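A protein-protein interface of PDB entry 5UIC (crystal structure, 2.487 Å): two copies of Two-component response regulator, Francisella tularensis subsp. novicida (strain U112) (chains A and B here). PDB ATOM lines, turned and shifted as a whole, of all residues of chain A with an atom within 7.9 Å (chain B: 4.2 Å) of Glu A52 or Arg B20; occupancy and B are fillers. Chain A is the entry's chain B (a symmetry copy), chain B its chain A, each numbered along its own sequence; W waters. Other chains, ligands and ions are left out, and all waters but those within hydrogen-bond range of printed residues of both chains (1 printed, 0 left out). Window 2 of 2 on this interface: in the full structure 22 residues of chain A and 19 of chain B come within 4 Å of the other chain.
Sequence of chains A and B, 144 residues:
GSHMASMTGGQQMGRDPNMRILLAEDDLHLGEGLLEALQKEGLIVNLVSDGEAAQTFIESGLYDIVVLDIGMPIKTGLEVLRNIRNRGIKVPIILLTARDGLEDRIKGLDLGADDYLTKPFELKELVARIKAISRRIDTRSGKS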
ATOM      1  N   VAL A  48      -6.990  -9.819   2.980  1.00  0.00           N
ATOM      2  CA  VAL A  48      -7.956  -8.786   2.630  1.00  0.00           C
ATOM      3  C   VAL A  48      -7.377  -7.978   1.474  1.00  0.00           C
ATOM      4  O   VAL A  48      -6.193  -8.083   1.149  1.00  0.00           O
ATOM      5  CB  VAL A  48      -8.301  -7.860   3.820  1.00  0.00           C
ATOM      6  CG1 VAL A  48      -9.003  -8.639   4.919  1.00  0.00           C
ATOM      7  CG2 VAL A  48      -7.046  -7.182   4.354  1.00  0.00           C
ATOM      8  N   SER A  49      -8.229  -7.158   0.852  1.00  0.00           N
ATOM      9  CA  SER A  49      -7.829  -6.438  -0.349  1.00  0.00           C
ATOM     10  C   SER A  49      -8.322  -4.994  -0.396  1.00  0.00           C
ATOM     11  O   SER A  49      -8.250  -4.369  -1.461  1.00  0.00           O
ATOM     12  CB  SER A  49      -8.324  -7.186  -1.592  1.00  0.00           C
ATOM     13  OG  SER A  49      -9.704  -7.492  -1.487  1.00  0.00           O
ATOM     14  N   ASP A  50      -8.813  -4.437   0.710  1.00  0.00           N
ATOM     15  CA  ASP A  50      -9.222  -3.043   0.734  1.00  0.00           C
ATOM     16  C   ASP A  50      -8.919  -2.456   2.104  1.00  0.00           C
ATOM     17  O   ASP A  50      -8.976  -3.153   3.122  1.00  0.00           O
ATOM     18  CB  ASP A  50     -10.711  -2.881   0.394  1.00  0.00           C
ATOM     19  CG  ASP A  50     -11.619  -3.324   1.520  1.00  0.00           C
ATOM     20  OD1 ASP A  50     -11.755  -2.569   2.506  1.00  0.00           O
ATOM     21  OD2 ASP A  50     -12.195  -4.428   1.420  1.00  0.00           O
ATOM     22  N   GLY A  51      -8.598  -1.162   2.117  1.00  0.00           N
ATOM     23  CA  GLY A  51      -8.150  -0.521   3.343  1.00  0.00           C
ATOM     24  C   GLY A  51      -9.174  -0.553   4.457  1.00  0.00           C
ATOM     25  O   GLY A  51      -8.810  -0.640   5.633  1.00  0.00           O
ATOM     26  N   GLU A  52     -10.461  -0.473   4.117  1.00  0.00           N
ATOM     27  CA  GLU A  52     -11.491  -0.465   5.151  1.00  0.00           C
ATOM     28  C   GLU A  52     -11.486  -1.774   5.930  1.00  0.00           C
ATOM     29  O   GLU A  52     -11.538  -1.777   7.165  1.00  0.00           O
ATOM     30  CB  GLU A  52     -12.865  -0.215   4.531  1.00  0.00           C
ATOM     31  CG  GLU A  52     -13.987  -0.111   5.554  1.00  0.00           C
ATOM     32  CD  GLU A  52     -15.323   0.242   4.927  1.00  0.00           C
ATOM     33  OE1 GLU A  52     -15.450   0.133   3.689  1.00  0.00           O
ATOM     34  OE2 GLU A  52     -16.246   0.632   5.673  1.00  0.00           O
ATOM     35  N   ALA A  53     -11.422  -2.901   5.222  1.00  0.00           N
ATOM     36  CA  ALA A  53     -11.371  -4.194   5.895  1.00  0.00           C
ATOM     37  C   ALA A  53     -10.039  -4.392   6.609  1.00  0.00           C
ATOM     38  O   ALA A  53      -9.995  -4.968   7.701  1.00  0.00           O
ATOM     39  CB  ALA A  53     -11.615  -5.319   4.890  1.00  0.00           C
ATOM     40  N   ALA A  54      -8.944  -3.920   6.008  1.00  0.00           N
ATOM     41  CA  ALA A  54      -7.637  -4.051   6.647  1.00  0.00           C
ATOM     42  C   ALA A  54      -7.616  -3.353   8.000  1.00  0.00           C
ATOM     43  O   ALA A  54      -7.120  -3.908   8.988  1.00  0.00           O
ATOM     44  CB  ALA A  54      -6.547  -3.486   5.738  1.00  0.00           C
ATOM     45  N   GLN A  55      -8.155  -2.135   8.068  1.00  0.00           N
ATOM     46  CA  GLN A  55      -8.179  -1.406   9.331  1.00  0.00           C
ATOM     47  C   GLN A  55      -9.015  -2.137  10.372  1.00  0.00           C
ATOM     48  O   GLN A  55      -8.622  -2.230  11.541  1.00  0.00           O
ATOM     49  CB  GLN A  55      -8.718   0.004   9.104  1.00  0.00           C
ATOM     50  CG  GLN A  55      -9.035   0.763  10.383  1.00  0.00           C
ATOM     51  CD  GLN A  55      -9.440   2.196  10.121  1.00  0.00           C
ATOM     52  OE1 GLN A  55      -9.417   2.665   8.983  1.00  0.00           O
ATOM     53  NE2 GLN A  55      -9.819   2.903  11.178  1.00  0.00           N
ATOM     54  N   THR A  56     -10.173  -2.661   9.969  1.00  0.00           N
ATOM     55  CA  THR A  56     -11.029  -3.371  10.915  1.00  0.00           C
ATOM     56  C   THR A  56     -10.351  -4.637  11.420  1.00  0.00           C
ATOM     57  O   THR A  56     -10.431  -4.959  12.611  1.00  0.00           O
ATOM     58  CB  THR A  56     -12.373  -3.705  10.259  1.00  0.00           C
ATOM     59  OG1 THR A  56     -12.890  -2.544   9.595  1.00  0.00           O
ATOM     60  CG2 THR A  56     -13.375  -4.163  11.302  1.00  0.00           C
ATOM     61  N   PHE A  57      -9.683  -5.371  10.528  1.00  0.00           N
ATOM     62  CA  PHE A  57      -8.945  -6.557  10.946  1.00  0.00           C
ATOM     63  C   PHE A  57      -7.842  -6.190  11.933  1.00  0.00           C
ATOM     64  O   PHE A  57      -7.692  -6.824  12.983  1.00  0.00           O
ATOM     65  CB  PHE A  57      -8.357  -7.260   9.722  1.00  0.00           C
ATOM     66  CG  PHE A  57      -9.328  -8.157   9.005  1.00  0.00           C
ATOM     67  CD1 PHE A  57     -10.576  -7.693   8.616  1.00  0.00           C
ATOM     68  CD2 PHE A  57      -8.982  -9.465   8.704  1.00  0.00           C
ATOM     69  CE1 PHE A  57     -11.460  -8.521   7.953  1.00  0.00           C
ATOM     70  CE2 PHE A  57      -9.862 -10.296   8.034  1.00  0.00           C
ATOM     71  CZ  PHE A  57     -11.100  -9.825   7.661  1.00  0.00           C
ATOM     72  N   ILE A  58      -7.057  -5.165  11.605  1.00  0.00           N
ATOM     73  CA  ILE A  58      -5.959  -4.750  12.473  1.00  0.00           C
ATOM     74  C   ILE A  58      -6.487  -4.346  13.843  1.00  0.00           C
ATOM     75  O   ILE A  58      -5.920  -4.716  14.878  1.00  0.00           O
ATOM     76  CB  ILE A  58      -5.172  -3.606  11.809  1.00  0.00           C
ATOM     77  CG1 ILE A  58      -4.501  -4.104  10.524  1.00  0.00           C
ATOM     78  CG2 ILE A  58      -4.132  -3.039  12.769  1.00  0.00           C
ATOM     79  CD1 ILE A  58      -4.058  -2.992   9.597  1.00  0.00           C
ATOM     80  N   GLU A  59      -7.577  -3.575  13.872  1.00  0.00           N
ATOM     81  CA  GLU A  59      -8.123  -3.107  15.141  1.00  0.00           C
ATOM     82  C   GLU A  59      -8.590  -4.260  16.018  1.00  0.00           C
ATOM     83  O   GLU A  59      -8.615  -4.134  17.249  1.00  0.00           O
ATOM     84  CB  GLU A  59      -9.279  -2.139  14.886  1.00  0.00           C
ATOM     85  CG  GLU A  59      -8.835  -0.750  14.459  1.00  0.00           C
ATOM     86  CD  GLU A  59      -9.994   0.118  13.997  1.00  0.00           C
ATOM     87  OE1 GLU A  59     -11.059  -0.441  13.658  1.00  0.00           O
ATOM     88  OE2 GLU A  59      -9.839   1.357  13.976  1.00  0.00           O
ATOM     89  N   MET A  72      -4.055   0.704  -1.408  1.00  0.00           N
ATOM     90  CA  MET A  72      -5.279  -0.075  -1.362  1.00  0.00           C
ATOM     91  C   MET A  72      -6.470   0.755  -1.821  1.00  0.00           C
ATOM     92  O   MET A  72      -6.424   1.987  -1.816  1.00  0.00           O
ATOM     93  CB  MET A  72      -5.544  -0.571   0.052  1.00  0.00           C
ATOM     94  CG  MET A  72      -4.381  -1.276   0.690  1.00  0.00           C
ATOM     95  SD  MET A  72      -4.905  -2.449   1.950  1.00  0.00           S
ATOM     96  CE  MET A  72      -5.575  -3.754   0.928  1.00  0.00           C
ATOM     97  N   PRO A  73      -7.559   0.105  -2.217  1.00  0.00           N
ATOM     98  CA  PRO A  73      -8.800   0.840  -2.463  1.00  0.00           C
ATOM     99  C   PRO A  73      -9.415   1.349  -1.169  1.00  0.00           C
ATOM    100  O   PRO A  73      -9.106   0.883  -0.070  1.00  0.00           O
ATOM    101  CB  PRO A  73      -9.710  -0.190  -3.138  1.00  0.00           C
ATOM    102  CG  PRO A  73      -8.780  -1.259  -3.638  1.00  0.00           C
ATOM    103  CD  PRO A  73      -7.649  -1.294  -2.670  1.00  0.00           C
ATOM    104  N   ILE A  74     -10.301   2.328  -1.327  1.00  0.00           N
ATOM    105  CA  ILE A  74     -11.010   2.951  -0.218  1.00  0.00           C
ATOM    106  C   ILE A  74     -10.001   3.727   0.620  1.00  0.00           C
ATOM    107  O   ILE A  74      -9.777   4.921   0.384  1.00  0.00           O
ATOM    108  CB  ILE A  74     -11.779   1.916   0.626  1.00  0.00           C
ATOM    109  CG1 ILE A  74     -12.724   1.100  -0.263  1.00  0.00           C
ATOM    110  CG2 ILE A  74     -12.559   2.623   1.728  1.00  0.00           C
ATOM    111  CD1 ILE A  74     -13.377  -0.048   0.450  1.00  0.00           C
ATOM    112  N   LYS A  75      -9.378   3.067   1.590  1.00  0.00           N
ATOM    113  CA  LYS A  75      -8.360   3.684   2.432  1.00  0.00           C
ATOM    114  C   LYS A  75      -6.992   3.168   2.013  1.00  0.00           C
ATOM    115  O   LYS A  75      -6.791   1.955   1.895  1.00  0.00           O
ATOM    116  CB  LYS A  75      -8.596   3.382   3.913  1.00  0.00           C
ATOM    117  CG  LYS A  75     -10.021   3.623   4.395  1.00  0.00           C
ATOM    118  CD  LYS A  75     -10.103   3.627   5.918  1.00  0.00           C
ATOM    119  CE  LYS A  75     -11.542   3.674   6.402  1.00  0.00           C
ATOM    120  NZ  LYS A  75     -11.607   3.848   7.877  1.00  0.00           N
ATOM    121  N   THR A  76      -6.057   4.085   1.785  1.00  0.00           N
ATOM    122  CA  THR A  76      -4.709   3.671   1.434  1.00  0.00           C
ATOM    123  C   THR A  76      -4.012   3.077   2.654  1.00  0.00           C
ATOM    124  O   THR A  76      -4.497   3.154   3.786  1.00  0.00           O
ATOM    125  CB  THR A  76      -3.901   4.850   0.892  1.00  0.00           C
ATOM    126  OG1 THR A  76      -3.566   5.736   1.964  1.00  0.00           O
ATOM    127  CG2 THR A  76      -4.693   5.609  -0.164  1.00  0.00           C
ATOM    128  N   VAL A  80      -4.693   3.828   6.780  1.00  0.00           N
ATOM    129  CA  VAL A  80      -4.881   2.733   7.730  1.00  0.00           C
ATOM    130  C   VAL A  80      -3.826   2.806   8.822  1.00  0.00           C
ATOM    131  O   VAL A  80      -4.129   2.695  10.016  1.00  0.00           O
ATOM    132  CB  VAL A  80      -4.840   1.382   6.995  1.00  0.00           C
ATOM    133  CG1 VAL A  80      -4.900   0.229   7.986  1.00  0.00           C
ATOM    134  CG2 VAL A  80      -5.986   1.285   5.995  1.00  0.00           C
ATOM    135  N   ASN B  18     -17.741  -2.027  -2.727  1.00  0.00           N
ATOM    136  CA  ASN B  18     -18.639  -2.968  -3.458  1.00  0.00           C
ATOM    137  C   ASN B  18     -18.921  -4.205  -2.601  1.00  0.00           C
ATOM    138  O   ASN B  18     -18.888  -4.135  -1.371  1.00  0.00           O
ATOM    139  CB  ASN B  18     -18.023  -3.362  -4.806  1.00  0.00           C
ATOM    140  CG  ASN B  18     -17.841  -2.176  -5.732  1.00  0.00           C
ATOM    141  OD1 ASN B  18     -18.366  -1.089  -5.483  1.00  0.00           O
ATOM    142  ND2 ASN B  18     -17.103  -2.381  -6.817  1.00  0.00           N
ATOM    143  N   MET B  19     -19.206  -5.332  -3.249  1.00  0.00           N
ATOM    144  CA  MET B  19     -19.576  -6.550  -2.543  1.00  0.00           C
ATOM    145  C   MET B  19     -18.336  -7.279  -2.034  1.00  0.00           C
ATOM    146  O   MET B  19     -17.320  -7.367  -2.730  1.00  0.00           O
ATOM    147  CB  MET B  19     -20.387  -7.458  -3.468  1.00  0.00           C
ATOM    148  CG  MET B  19     -20.705  -8.833  -2.899  1.00  0.00           C
ATOM    149  SD  MET B  19     -21.747  -9.820  -3.994  1.00  0.00           S
ATOM    150  CE  MET B  19     -23.259  -8.857  -4.002  1.00  0.00           C
ATOM    151  N   ARG B  20     -18.428  -7.810  -0.813  1.00  0.00           N
ATOM    152  CA  ARG B  20     -17.328  -8.520  -0.176  1.00  0.00           C
ATOM    153  C   ARG B  20     -17.786  -9.902   0.264  1.00  0.00           C
ATOM    154  O   ARG B  20     -18.893 -10.061   0.788  1.00  0.00           O
ATOM    155  CB  ARG B  20     -16.790  -7.752   1.038  1.00  0.00           C
ATOM    156  CG  ARG B  20     -15.628  -6.817   0.732  1.00  0.00           C
ATOM    157  CD  ARG B  20     -15.071  -6.208   2.012  1.00  0.00           C
ATOM    158  NE  ARG B  20     -16.035  -5.311   2.648  1.00  0.00           N
ATOM    159  CZ  ARG B  20     -15.917  -3.987   2.734  1.00  0.00           C
ATOM    160  NH1 ARG B  20     -14.858  -3.354   2.240  1.00  0.00           N
ATOM    161  NH2 ARG B  20     -16.871  -3.284   3.332  1.00  0.00           N
ATOM    162  N   ILE B  21     -16.925 -10.895   0.056  1.00  0.00           N
ATOM    163  CA  ILE B  21     -17.187 -12.273   0.454  1.00  0.00           C
ATOM    164  C   ILE B  21     -16.105 -12.706   1.433  1.00  0.00           C
ATOM    165  O   ILE B  21     -14.911 -12.541   1.159  1.00  0.00           O
ATOM    166  CB  ILE B  21     -17.230 -13.219  -0.761  1.00  0.00           C
ATOM    167  CG1 ILE B  21     -18.329 -12.778  -1.732  1.00  0.00           C
ATOM    168  CG2 ILE B  21     -17.463 -14.661  -0.303  1.00  0.00           C
ATOM    169  CD1 ILE B  21     -18.367 -13.555  -3.032  1.00  0.00           C
ATOM    170  N   ILE B  44     -14.904  -9.484  -4.698  1.00  0.00           N
ATOM    171  CA  ILE B  44     -13.911  -9.226  -3.663  1.00  0.00           C
ATOM    172  C   ILE B  44     -14.040 -10.300  -2.594  1.00  0.00           C
ATOM    173  O   ILE B  44     -15.143 -10.570  -2.102  1.00  0.00           O
ATOM    174  CB  ILE B  44     -14.099  -7.820  -3.068  1.00  0.00           C
ATOM    175  CG1 ILE B  44     -13.886  -6.751  -4.145  1.00  0.00           C
ATOM    176  CG2 ILE B  44     -13.160  -7.594  -1.891  1.00  0.00           C
ATOM    177  CD1 ILE B  44     -12.493  -6.738  -4.755  1.00  0.00           C
ATOM    178  N   ASN B  46     -12.139 -12.205   0.922  1.00  0.00           N
ATOM    179  CA  ASN B  46     -11.183 -12.247   2.016  1.00  0.00           C
ATOM    180  C   ASN B  46     -11.165 -13.649   2.610  1.00  0.00           C
ATOM    181  O   ASN B  46     -12.123 -14.414   2.469  1.00  0.00           O
ATOM    182  CB  ASN B  46     -11.530 -11.213   3.095  1.00  0.00           C
ATOM    183  CG  ASN B  46     -11.542  -9.793   2.557  1.00  0.00           C
ATOM    184  OD1 ASN B  46     -10.997  -9.517   1.489  1.00  0.00           O
ATOM    185  ND2 ASN B  46     -12.161  -8.883   3.299  1.00  0.00           N
ATOM    186  N   LEU B  62     -19.008  -5.880   7.346  1.00  0.00           N
ATOM    187  CA  LEU B  62     -18.302  -5.569   6.110  1.00  0.00           C
ATOM    188  C   LEU B  62     -18.646  -6.513   4.968  1.00  0.00           C
ATOM    189  O   LEU B  62     -18.298  -6.215   3.820  1.00  0.00           O
ATOM    190  CB  LEU B  62     -16.789  -5.616   6.330  1.00  0.00           C
ATOM    191  CG  LEU B  62     -16.142  -4.429   7.043  1.00  0.00           C
ATOM    192  CD1 LEU B  62     -16.049  -4.692   8.530  1.00  0.00           C
ATOM    193  CD2 LEU B  62     -14.771  -4.149   6.457  1.00  0.00           C
ATOM    194  N   TYR B  63     -19.310  -7.630   5.242  1.00  0.00           N
ATOM    195  CA  TYR B  63     -19.447  -8.702   4.269  1.00  0.00           C
ATOM    196  C   TYR B  63     -20.895  -8.878   3.839  1.00  0.00           C
ATOM    197  O   TYR B  63     -21.821  -8.742   4.645  1.00  0.00           O
ATOM    198  CB  TYR B  63     -18.898 -10.008   4.837  1.00  0.00           C
ATOM    199  CG  TYR B  63     -17.405  -9.949   4.997  1.00  0.00           C
ATOM    200  CD1 TYR B  63     -16.572 -10.055   3.894  1.00  0.00           C
ATOM    201  CD2 TYR B  63     -16.824  -9.751   6.242  1.00  0.00           C
ATOM    202  CE1 TYR B  63     -15.211  -9.984   4.024  1.00  0.00           C
ATOM    203  CE2 TYR B  63     -15.460  -9.680   6.381  1.00  0.00           C
ATOM    204  CZ  TYR B  63     -14.659  -9.796   5.269  1.00  0.00           C
ATOM    205  OH  TYR B  63     -13.294  -9.723   5.404  1.00  0.00           O
ATOM    206  N   ASP B  64     -21.069  -9.180   2.554  1.00  0.00           N
ATOM    207  CA  ASP B  64     -22.377  -9.401   1.965  1.00  0.00           C
ATOM    208  C   ASP B  64     -22.696 -10.875   1.773  1.00  0.00           C
ATOM    209  O   ASP B  64     -23.874 -11.231   1.688  1.00  0.00           O
ATOM    210  CB  ASP B  64     -22.456  -8.681   0.617  1.00  0.00           C
ATOM    211  CG  ASP B  64     -22.071  -7.217   0.722  1.00  0.00           C
ATOM    212  OD1 ASP B  64     -22.876  -6.421   1.250  1.00  0.00           O
ATOM    213  OD2 ASP B  64     -20.948  -6.868   0.300  1.00  0.00           O
ATOM    214  N   ILE B  65     -21.679 -11.728   1.689  1.00  0.00           N
ATOM    215  CA  ILE B  65     -21.853 -13.175   1.656  1.00  0.00           C
ATOM    216  C   ILE B  65     -20.729 -13.797   2.471  1.00  0.00           C
ATOM    217  O   ILE B  65     -19.592 -13.313   2.455  1.00  0.00           O
ATOM    218  CB  ILE B  65     -21.856 -13.729   0.216  1.00  0.00           C
ATOM    219  CG1 ILE B  65     -22.937 -13.038  -0.616  1.00  0.00           C
ATOM    220  CG2 ILE B  65     -22.080 -15.239   0.229  1.00  0.00           C
ATOM    221  CD1 ILE B  65     -23.016 -13.519  -2.047  1.00  0.00           C
HETATM  222  O   HOH W   1     -10.880  -6.902   1.350  1.00  0.00           O
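Hydrophobic or aromatic side chains of chain A within 4 Å of the printed part of chain B: Val A48, Ala A53 and Phe A57.
Hydrophobic or aromatic side chains of chain B that line the printed part of chain A: Ile B44, Leu B62 and Tyr B63.
Among the printed residues, Asp or Glu carboxylates within 4 Å of a Lys or Arg side-chain nitrogen of the other chain: Asp A50 with Arg B20 (3.0 Å) and Glu A52 with Arg B20 (3.7 Å).
No position is printed for both chains.
Water W1 lies within hydrogen-bond range of the side-chain amide oxygen of Asn B46 (2.6 Å), the backbone NH of Ser A49 (2.7 Å) and the side-chain carboxylate of Asp A50 (2.8 Å).
Among the printed residues, pairs that only touch across the chains: Val A48 with Asn B46 (3.3 Å), Ser A49 with Ile B44 (3.5 Å), Ser A49 with Asn B46 (3.7 Å), Ala A53 with Asn B46 (3.9 Å), Ala A53 with Leu B62 (3.4 Å), Thr A56 with Leu B62 (3.9 Å) and Phe A57 with Tyr B63 (3.1 Å).
Glu A52 touches one residue of chain B.
Of chain A, only Asp A50 and Glu A52 come within 4 Å of Arg B20.
Printed residues of chain B within 4 Å of Thr A56: Leu B62 (3.9 Å).
Printed residues of chain B within 4 Å of Ser A49: Ile B44 (3.5 Å) and Asn B46 (3.7 Å).
Pro A73 touches none of the printed residues of chain B.
The nearest residue of chain B that does not touch Glu A52 is Leu B62 (4.1 Å).
The guanidinium group of Arg B20 lies within salt-bridge range of the side-chain carboxylate of Glu A52 (3.7 Å).
OD2 of Asp A50 lies within salt-bridge range of NH1 of Arg B20, at 3.0 Å.
N of Ala A53 lies within hydrogen-bond range of OD1 of Asp A50, 2.8 Å away.
The backbone NH (N) of Asn B46 is in hydrogen-bond range of the backbone carbonyl oxygen (O) of Ile B21.
The side-chain carboxylate (OD1) of Asp A50 lies within hydrogen-bond range of the backbone NH (N) of Glu A52 (2.9 Å).
The side-chain carboxylate (OD2) of Asp B64 lies within hydrogen-bond range of the backbone NH (N) of Arg B20, at 2.9 Å.
ND2 of Asn B46 sits at hydrogen-bond distance from OH of Tyr B63 (2.5 Å).
The backbone carbonyl oxygen of Leu B62 is in hydrogen-bond range of the guanidinium group of Arg B20 (2.7 Å).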
